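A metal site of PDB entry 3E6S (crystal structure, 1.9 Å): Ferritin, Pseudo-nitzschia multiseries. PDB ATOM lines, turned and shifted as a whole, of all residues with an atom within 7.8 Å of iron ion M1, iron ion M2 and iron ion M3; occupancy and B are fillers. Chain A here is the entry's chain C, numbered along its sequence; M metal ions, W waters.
OH of Tyr 23 lies close to OE1 of Glu 45 (3.3 Å). The side-chain hydroxyl (OH) of Tyr 23 sits close to the side-chain carboxylate (OE2) of Glu 95 (2.6 Å). The side-chain carboxylate of Glu 95 sits close to the side-chain amide oxygen of Gln 128. ND2 of Asn 98 sits at hydrogen-bond distance from OE1 of Glu 95. The side-chain carboxylate (OE2) of Glu 48 lies close to the side-chain amide nitrogen (NE2) of Gln 127 (2.8 Å). The backbone carbonyl oxygen of Glu 48 lies within hydrogen-bond range of a ring nitrogen (ND1) of His 52 (3.3 Å). The side-chain amide oxygen (OE1) of Gln 127 is in hydrogen-bond range of a ring nitrogen (NE2) of His 52 (3.0 Å).
The side-chain carboxylate (OE2) of Glu 49 binds iron ion M1, at 1.9 Å. OE2 of Glu 95 binds iron ion M1 (2.1 Å). Iron ion M1 is bound by water W1, at 2.2 Å. Iron ion M1 is bound by water W2 (2.2 Å). Iron ion M1 is bound by OE1 of Glu 45, 2.2 Å away. The side-chain carboxylate (OE2) of Glu 131 binds iron ion M1, 2.5 Å away.
Iron ion M2 is bound by OE2 of Glu 45, OE2 of Glu 48, water W1 and water W3. Iron ion M2 has four donor atoms within binding distance. Slightly farther from iron ion M2 lies the side-chain carboxylate (OE2) of Glu 131 (2.7 Å). Slightly farther from iron ion M2 lies OE1 of Glu 131 (2.8 Å).
Water W2 lies within hydrogen-bond range of the side-chain carboxylate of Glu 95, the side-chain amide nitrogen of Gln 128 and the side-chain carboxylate of Glu 131.
Merely in contact with iron ion M1: Tyr 23 (3.9 Å). Within 4 Å of iron ion M1: Tyr 23, Glu 45, Glu 49, Glu 95 and Glu 131.
Merely in contact with iron ion M3: Gln 127 (3.5 Å). The nearest printed residue that does not touch iron ion M3 is Glu 131 (4.6 Å).
Of the 21 residues printed, 3 come within 4 Å of iron ion M2. Along chain A the residues within 4 Å of iron ion M2 span positions 45 to 131.
Iron ion M3 is bound by the side-chain carboxylate (OE2) of Glu 48 (2.6 Å) and the side-chain carboxylate (OE1) of Glu 48 (2.6 Å). Iron ion M3 has two donor atoms within binding distance. Slightly farther from iron ion M3 lies water W3 (2.6 Å).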
ATOM      1  N   GLU A  16       0.783   5.665  20.909  1.00  0.00           N
ATOM      2  CA  GLU A  16       1.133   6.792  21.778  1.00  0.00           C
ATOM      3  C   GLU A  16       2.619   6.791  22.107  1.00  0.00           C
ATOM      4  O   GLU A  16       3.278   7.850  22.085  1.00  0.00           O
ATOM      5  CB  GLU A  16       0.337   6.785  23.087  1.00  0.00           C
ATOM      6  CG  GLU A  16      -1.195   6.883  22.916  1.00  0.00           C
ATOM      7  CD  GLU A  16      -1.637   8.193  22.279  1.00  0.00           C
ATOM      8  OE1 GLU A  16      -0.969   9.241  22.487  1.00  0.00           O
ATOM      9  OE2 GLU A  16      -2.682   8.207  21.589  1.00  0.00           O
ATOM     10  N   ALA A  19       4.684   7.714  18.983  1.00  0.00           N
ATOM     11  CA  ALA A  19       4.611   9.163  18.876  1.00  0.00           C
ATOM     12  C   ALA A  19       5.543   9.890  19.883  1.00  0.00           C
ATOM     13  O   ALA A  19       6.268  10.831  19.519  1.00  0.00           O
ATOM     14  CB  ALA A  19       3.196   9.619  19.046  1.00  0.00           C
ATOM     15  N   TYR A  23       8.478  12.416  18.720  1.00  0.00           N
ATOM     16  CA  TYR A  23       8.668  13.778  19.286  1.00  0.00           C
ATOM     17  C   TYR A  23      10.043  13.945  19.894  1.00  0.00           C
ATOM     18  O   TYR A  23      10.657  14.999  19.732  1.00  0.00           O
ATOM     19  CB  TYR A  23       7.612  14.099  20.347  1.00  0.00           C
ATOM     20  CG  TYR A  23       6.346  14.670  19.776  1.00  0.00           C
ATOM     21  CD1 TYR A  23       6.319  15.975  19.250  1.00  0.00           C
ATOM     22  CD2 TYR A  23       5.173  13.922  19.760  1.00  0.00           C
ATOM     23  CE1 TYR A  23       5.134  16.529  18.727  1.00  0.00           C
ATOM     24  CE2 TYR A  23       3.969  14.477  19.231  1.00  0.00           C
ATOM     25  CZ  TYR A  23       3.974  15.786  18.738  1.00  0.00           C
ATOM     26  OH  TYR A  23       2.808  16.377  18.218  1.00  0.00           O
ATOM     27  N   TYR A  41       9.418  22.479  22.845  1.00  0.00           N
ATOM     28  CA  TYR A  41       8.041  22.141  22.483  1.00  0.00           C
ATOM     29  C   TYR A  41       7.919  20.639  22.173  1.00  0.00           C
ATOM     30  O   TYR A  41       7.025  19.955  22.680  1.00  0.00           O
ATOM     31  CB  TYR A  41       7.610  22.968  21.274  1.00  0.00           C
ATOM     32  CG  TYR A  41       6.159  22.798  20.905  1.00  0.00           C
ATOM     33  CD1 TYR A  41       5.206  23.699  21.360  1.00  0.00           C
ATOM     34  CD2 TYR A  41       5.736  21.714  20.149  1.00  0.00           C
ATOM     35  CE1 TYR A  41       3.895  23.543  21.046  1.00  0.00           C
ATOM     36  CE2 TYR A  41       4.424  21.537  19.838  1.00  0.00           C
ATOM     37  CZ  TYR A  41       3.501  22.460  20.298  1.00  0.00           C
ATOM     38  OH  TYR A  41       2.174  22.323  20.004  1.00  0.00           O
ATOM     39  N   ALA A  44       8.208  18.609  25.419  1.00  0.00           N
ATOM     40  CA  ALA A  44       6.939  18.629  26.145  1.00  0.00           C
ATOM     41  C   ALA A  44       5.908  17.658  25.554  1.00  0.00           C
ATOM     42  O   ALA A  44       5.242  16.903  26.297  1.00  0.00           O
ATOM     43  CB  ALA A  44       6.353  20.067  26.208  1.00  0.00           C
ATOM     44  N   GLU A  45       5.779  17.634  24.217  1.00  0.00           N
ATOM     45  CA  GLU A  45       4.842  16.689  23.582  1.00  0.00           C
ATOM     46  C   GLU A  45       5.276  15.249  23.773  1.00  0.00           C
ATOM     47  O   GLU A  45       4.441  14.329  23.896  1.00  0.00           O
ATOM     48  CB  GLU A  45       4.743  16.949  22.076  1.00  0.00           C
ATOM     49  CG  GLU A  45       3.744  17.979  21.710  1.00  0.00           C
ATOM     50  CD  GLU A  45       2.327  17.484  21.920  1.00  0.00           C
ATOM     51  OE1 GLU A  45       1.901  16.452  21.357  1.00  0.00           O
ATOM     52  OE2 GLU A  45       1.619  18.145  22.708  1.00  0.00           O
ATOM     53  N   SER A  46       6.587  15.018  23.737  1.00  0.00           N
ATOM     54  CA  SER A  46       7.080  13.671  24.005  1.00  0.00           C
ATOM     55  C   SER A  46       6.591  13.153  25.368  1.00  0.00           C
ATOM     56  O   SER A  46       6.131  12.016  25.469  1.00  0.00           O
ATOM     57  CB  SER A  46       8.614  13.629  23.940  1.00  0.00           C
ATOM     58  OG  SER A  46       9.063  12.281  24.144  1.00  0.00           O
ATOM     59  N   GLU A  48       3.966  14.286  27.097  1.00  0.00           N
ATOM     60  CA  GLU A  48       2.512  14.222  27.032  1.00  0.00           C
ATOM     61  C   GLU A  48       1.948  12.973  26.271  1.00  0.00           C
ATOM     62  O   GLU A  48       1.002  12.334  26.742  1.00  0.00           O
ATOM     63  CB  GLU A  48       1.988  15.530  26.424  1.00  0.00           C
ATOM     64  CG  GLU A  48       0.577  15.459  25.977  1.00  0.00           C
ATOM     65  CD  GLU A  48      -0.031  16.829  25.749  1.00  0.00           C
ATOM     66  OE1 GLU A  48       0.566  17.850  26.215  1.00  0.00           O
ATOM     67  OE2 GLU A  48      -1.119  16.879  25.098  1.00  0.00           O
ATOM     68  N   GLU A  49       2.530  12.636  25.123  1.00  0.00           N
ATOM     69  CA  GLU A  49       2.159  11.428  24.414  1.00  0.00           C
ATOM     70  C   GLU A  49       2.410  10.186  25.292  1.00  0.00           C
ATOM     71  O   GLU A  49       1.608   9.264  25.297  1.00  0.00           O
ATOM     72  CB  GLU A  49       2.970  11.257  23.102  1.00  0.00           C
ATOM     73  CG  GLU A  49       2.770  12.340  22.049  1.00  0.00           C
ATOM     74  CD  GLU A  49       1.345  12.406  21.494  1.00  0.00           C
ATOM     75  OE1 GLU A  49       0.616  11.389  21.541  1.00  0.00           O
ATOM     76  OE2 GLU A  49       0.951  13.460  20.962  1.00  0.00           O
ATOM     77  N   HIS A  52      -0.402  10.051  27.753  1.00  0.00           N
ATOM     78  CA  HIS A  52      -1.560   9.515  27.063  1.00  0.00           C
ATOM     79  C   HIS A  52      -1.485   7.994  27.019  1.00  0.00           C
ATOM     80  O   HIS A  52      -2.468   7.307  27.361  1.00  0.00           O
ATOM     81  CB  HIS A  52      -1.710  10.081  25.645  1.00  0.00           C
ATOM     82  CG  HIS A  52      -2.031  11.549  25.607  1.00  0.00           C
ATOM     83  ND1 HIS A  52      -2.257  12.302  26.748  1.00  0.00           N
ATOM     84  CD2 HIS A  52      -2.155  12.414  24.562  1.00  0.00           C
ATOM     85  CE1 HIS A  52      -2.523  13.550  26.416  1.00  0.00           C
ATOM     86  NE2 HIS A  52      -2.461  13.651  25.091  1.00  0.00           N
ATOM     87  N   ILE A  91       5.601  16.026  12.056  1.00  0.00           N
ATOM     88  CA  ILE A  91       4.858  16.065  13.321  1.00  0.00           C
ATOM     89  C   ILE A  91       3.350  16.203  13.022  1.00  0.00           C
ATOM     90  O   ILE A  91       2.523  15.515  13.629  1.00  0.00           O
ATOM     91  CB  ILE A  91       5.410  17.160  14.247  1.00  0.00           C
ATOM     92  CG1 ILE A  91       6.827  16.781  14.742  1.00  0.00           C
ATOM     93  CG2 ILE A  91       4.456  17.499  15.428  1.00  0.00           C
ATOM     94  CD1 ILE A  91       6.974  15.424  15.329  1.00  0.00           C
ATOM     95  N   LEU A  94       2.159  12.942  12.014  1.00  0.00           N
ATOM     96  CA  LEU A  94       2.144  12.057  13.188  1.00  0.00           C
ATOM     97  C   LEU A  94       0.824  12.227  13.939  1.00  0.00           C
ATOM     98  O   LEU A  94       0.151  11.246  14.311  1.00  0.00           O
ATOM     99  CB  LEU A  94       3.385  12.367  14.087  1.00  0.00           C
ATOM    100  CG  LEU A  94       3.437  11.599  15.424  1.00  0.00           C
ATOM    101  CD1 LEU A  94       3.731  10.098  15.183  1.00  0.00           C
ATOM    102  CD2 LEU A  94       4.447  12.200  16.344  1.00  0.00           C
ATOM    103  N   GLU A  95       0.439  13.476  14.152  1.00  0.00           N
ATOM    104  CA  GLU A  95      -0.781  13.781  14.907  1.00  0.00           C
ATOM    105  C   GLU A  95      -2.026  13.428  14.104  1.00  0.00           C
ATOM    106  O   GLU A  95      -3.026  12.985  14.681  1.00  0.00           O
ATOM    107  CB  GLU A  95      -0.840  15.260  15.350  1.00  0.00           C
ATOM    108  CG  GLU A  95       0.108  15.635  16.476  1.00  0.00           C
ATOM    109  CD  GLU A  95      -0.221  14.984  17.832  1.00  0.00           C
ATOM    110  OE1 GLU A  95      -1.288  14.317  17.991  1.00  0.00           O
ATOM    111  OE2 GLU A  95       0.620  15.137  18.760  1.00  0.00           O
ATOM    112  N   ASN A  98      -2.319   9.836  14.682  1.00  0.00           N
ATOM    113  CA  ASN A  98      -2.828   9.687  16.054  1.00  0.00           C
ATOM    114  C   ASN A  98      -4.378   9.835  16.020  1.00  0.00           C
ATOM    115  O   ASN A  98      -5.123   8.987  16.527  1.00  0.00           O
ATOM    116  CB  ASN A  98      -2.241  10.759  17.008  1.00  0.00           C
ATOM    117  CG  ASN A  98      -0.766  10.473  17.474  1.00  0.00           C
ATOM    118  OD1 ASN A  98      -0.220   9.363  17.305  1.00  0.00           O
ATOM    119  ND2 ASN A  98      -0.128  11.496  18.093  1.00  0.00           N
ATOM    120  N   GLN A 127      -8.948  16.904  22.297  1.00  0.00           N
ATOM    121  CA  GLN A 127      -7.534  17.337  22.366  1.00  0.00           C
ATOM    122  C   GLN A 127      -6.865  17.215  21.001  1.00  0.00           C
ATOM    123  O   GLN A 127      -6.097  18.094  20.631  1.00  0.00           O
ATOM    124  CB  GLN A 127      -6.784  16.513  23.432  1.00  0.00           C
ATOM    125  CG  GLN A 127      -5.328  16.916  23.729  1.00  0.00           C
ATOM    126  CD  GLN A 127      -4.778  16.030  24.849  1.00  0.00           C
ATOM    127  OE1 GLN A 127      -5.176  14.848  24.989  1.00  0.00           O
ATOM    128  NE2 GLN A 127      -3.878  16.601  25.682  1.00  0.00           N
ATOM    129  N   GLN A 128      -7.155  16.146  20.247  1.00  0.00           N
ATOM    130  CA  GLN A 128      -6.608  16.004  18.875  1.00  0.00           C
ATOM    131  C   GLN A 128      -7.024  17.138  17.927  1.00  0.00           C
ATOM    132  O   GLN A 128      -6.241  17.554  17.050  1.00  0.00           O
ATOM    133  CB  GLN A 128      -6.996  14.684  18.233  1.00  0.00           C
ATOM    134  CG  GLN A 128      -6.243  13.438  18.757  1.00  0.00           C
ATOM    135  CD  GLN A 128      -4.727  13.691  18.773  1.00  0.00           C
ATOM    136  OE1 GLN A 128      -4.077  13.759  17.722  1.00  0.00           O
ATOM    137  NE2 GLN A 128      -4.194  13.913  19.947  1.00  0.00           N
ATOM    138  N   ASN A 130      -7.641  20.184  18.884  1.00  0.00           N
ATOM    139  CA  ASN A 130      -6.856  21.323  19.302  1.00  0.00           C
ATOM    140  C   ASN A 130      -5.434  21.177  18.820  1.00  0.00           C
ATOM    141  O   ASN A 130      -4.869  22.133  18.281  1.00  0.00           O
ATOM    142  CB  ASN A 130      -6.883  21.527  20.817  1.00  0.00           C
ATOM    143  CG  ASN A 130      -8.233  21.946  21.318  1.00  0.00           C
ATOM    144  OD1 ASN A 130      -9.076  22.422  20.542  1.00  0.00           O
ATOM    145  ND2 ASN A 130      -8.477  21.750  22.636  1.00  0.00           N
ATOM    146  N   GLU A 131      -4.880  19.972  18.971  1.00  0.00           N
ATOM    147  CA  GLU A 131      -3.465  19.769  18.634  1.00  0.00           C
ATOM    148  C   GLU A 131      -3.159  19.888  17.134  1.00  0.00           C
ATOM    149  O   GLU A 131      -2.193  20.534  16.781  1.00  0.00           O
ATOM    150  CB  GLU A 131      -2.929  18.438  19.160  1.00  0.00           C
ATOM    151  CG  GLU A 131      -2.993  18.352  20.679  1.00  0.00           C
ATOM    152  CD  GLU A 131      -1.920  17.424  21.260  1.00  0.00           C
ATOM    153  OE1 GLU A 131      -2.253  16.620  22.190  1.00  0.00           O
ATOM    154  OE2 GLU A 131      -0.747  17.511  20.799  1.00  0.00           O
ATOM    155  N   GLU A 132      -3.979  19.275  16.279  1.00  0.00           N
ATOM    156  CA  GLU A 132      -3.793  19.349  14.844  1.00  0.00           C
ATOM    157  C   GLU A 132      -3.888  20.809  14.399  1.00  0.00           C
ATOM    158  O   GLU A 132      -3.138  21.237  13.530  1.00  0.00           O
ATOM    159  CB  GLU A 132      -4.852  18.529  14.077  1.00  0.00           C
ATOM    160  CG  GLU A 132      -4.730  17.045  14.199  1.00  0.00           C
ATOM    161  CD  GLU A 132      -5.467  16.308  13.088  1.00  0.00           C
ATOM    162  OE1 GLU A 132      -5.714  16.891  12.016  1.00  0.00           O
ATOM    163  OE2 GLU A 132      -5.785  15.130  13.236  1.00  0.00           O
ATOM    164  N   LYS A 134      -3.189  23.497  16.257  1.00  0.00           N
ATOM    165  CA  LYS A 134      -1.980  24.207  16.751  1.00  0.00           C
ATOM    166  C   LYS A 134      -0.757  23.877  15.874  1.00  0.00           C
ATOM    167  O   LYS A 134      -0.004  24.780  15.482  1.00  0.00           O
ATOM    168  CB  LYS A 134      -1.661  23.844  18.218  1.00  0.00           C
ATOM    169  CG  LYS A 134      -0.628  24.790  18.843  1.00  0.00           C
ATOM    170  CD  LYS A 134      -0.124  24.361  20.246  1.00  0.00           C
ATOM    171  CE  LYS A 134       0.808  25.481  20.812  1.00  0.00           C
ATOM    172  NZ  LYS A 134       0.875  25.488  22.337  1.00  0.00           N
ATOM    173  N   ILE A 135      -0.574  22.586  15.570  1.00  0.00           N
ATOM    174  CA  ILE A 135       0.589  22.134  14.768  1.00  0.00           C
ATOM    175  C   ILE A 135       0.473  22.690  13.342  1.00  0.00           C
ATOM    176  O   ILE A 135       1.438  23.172  12.777  1.00  0.00           O
ATOM    177  CB  ILE A 135       0.746  20.566  14.694  1.00  0.00           C
ATOM    178  CG1 ILE A 135       0.855  19.886  16.083  1.00  0.00           C
ATOM    179  CG2 ILE A 135       1.973  20.203  13.843  1.00  0.00           C
ATOM    180  CD1 ILE A 135       1.829  20.541  17.016  1.00  0.00           C
HETATM  181 FE    FE M   1       0.157  15.232  20.851  1.00  0.00          FE
HETATM  182 FE    FE M   2      -0.129  17.963  23.345  1.00  0.00          FE
HETATM  183 FE    FE M   3      -1.579  19.275  25.911  1.00  0.00          FE
HETATM  184  O   HOH W   1      -0.249  15.610  22.937  1.00  0.00           O
HETATM  185  O   HOH W   2      -1.610  13.986  20.616  1.00  0.00           O
HETATM  186  O   HOH W   3       0.596  19.990  24.630  1.00  0.00           O
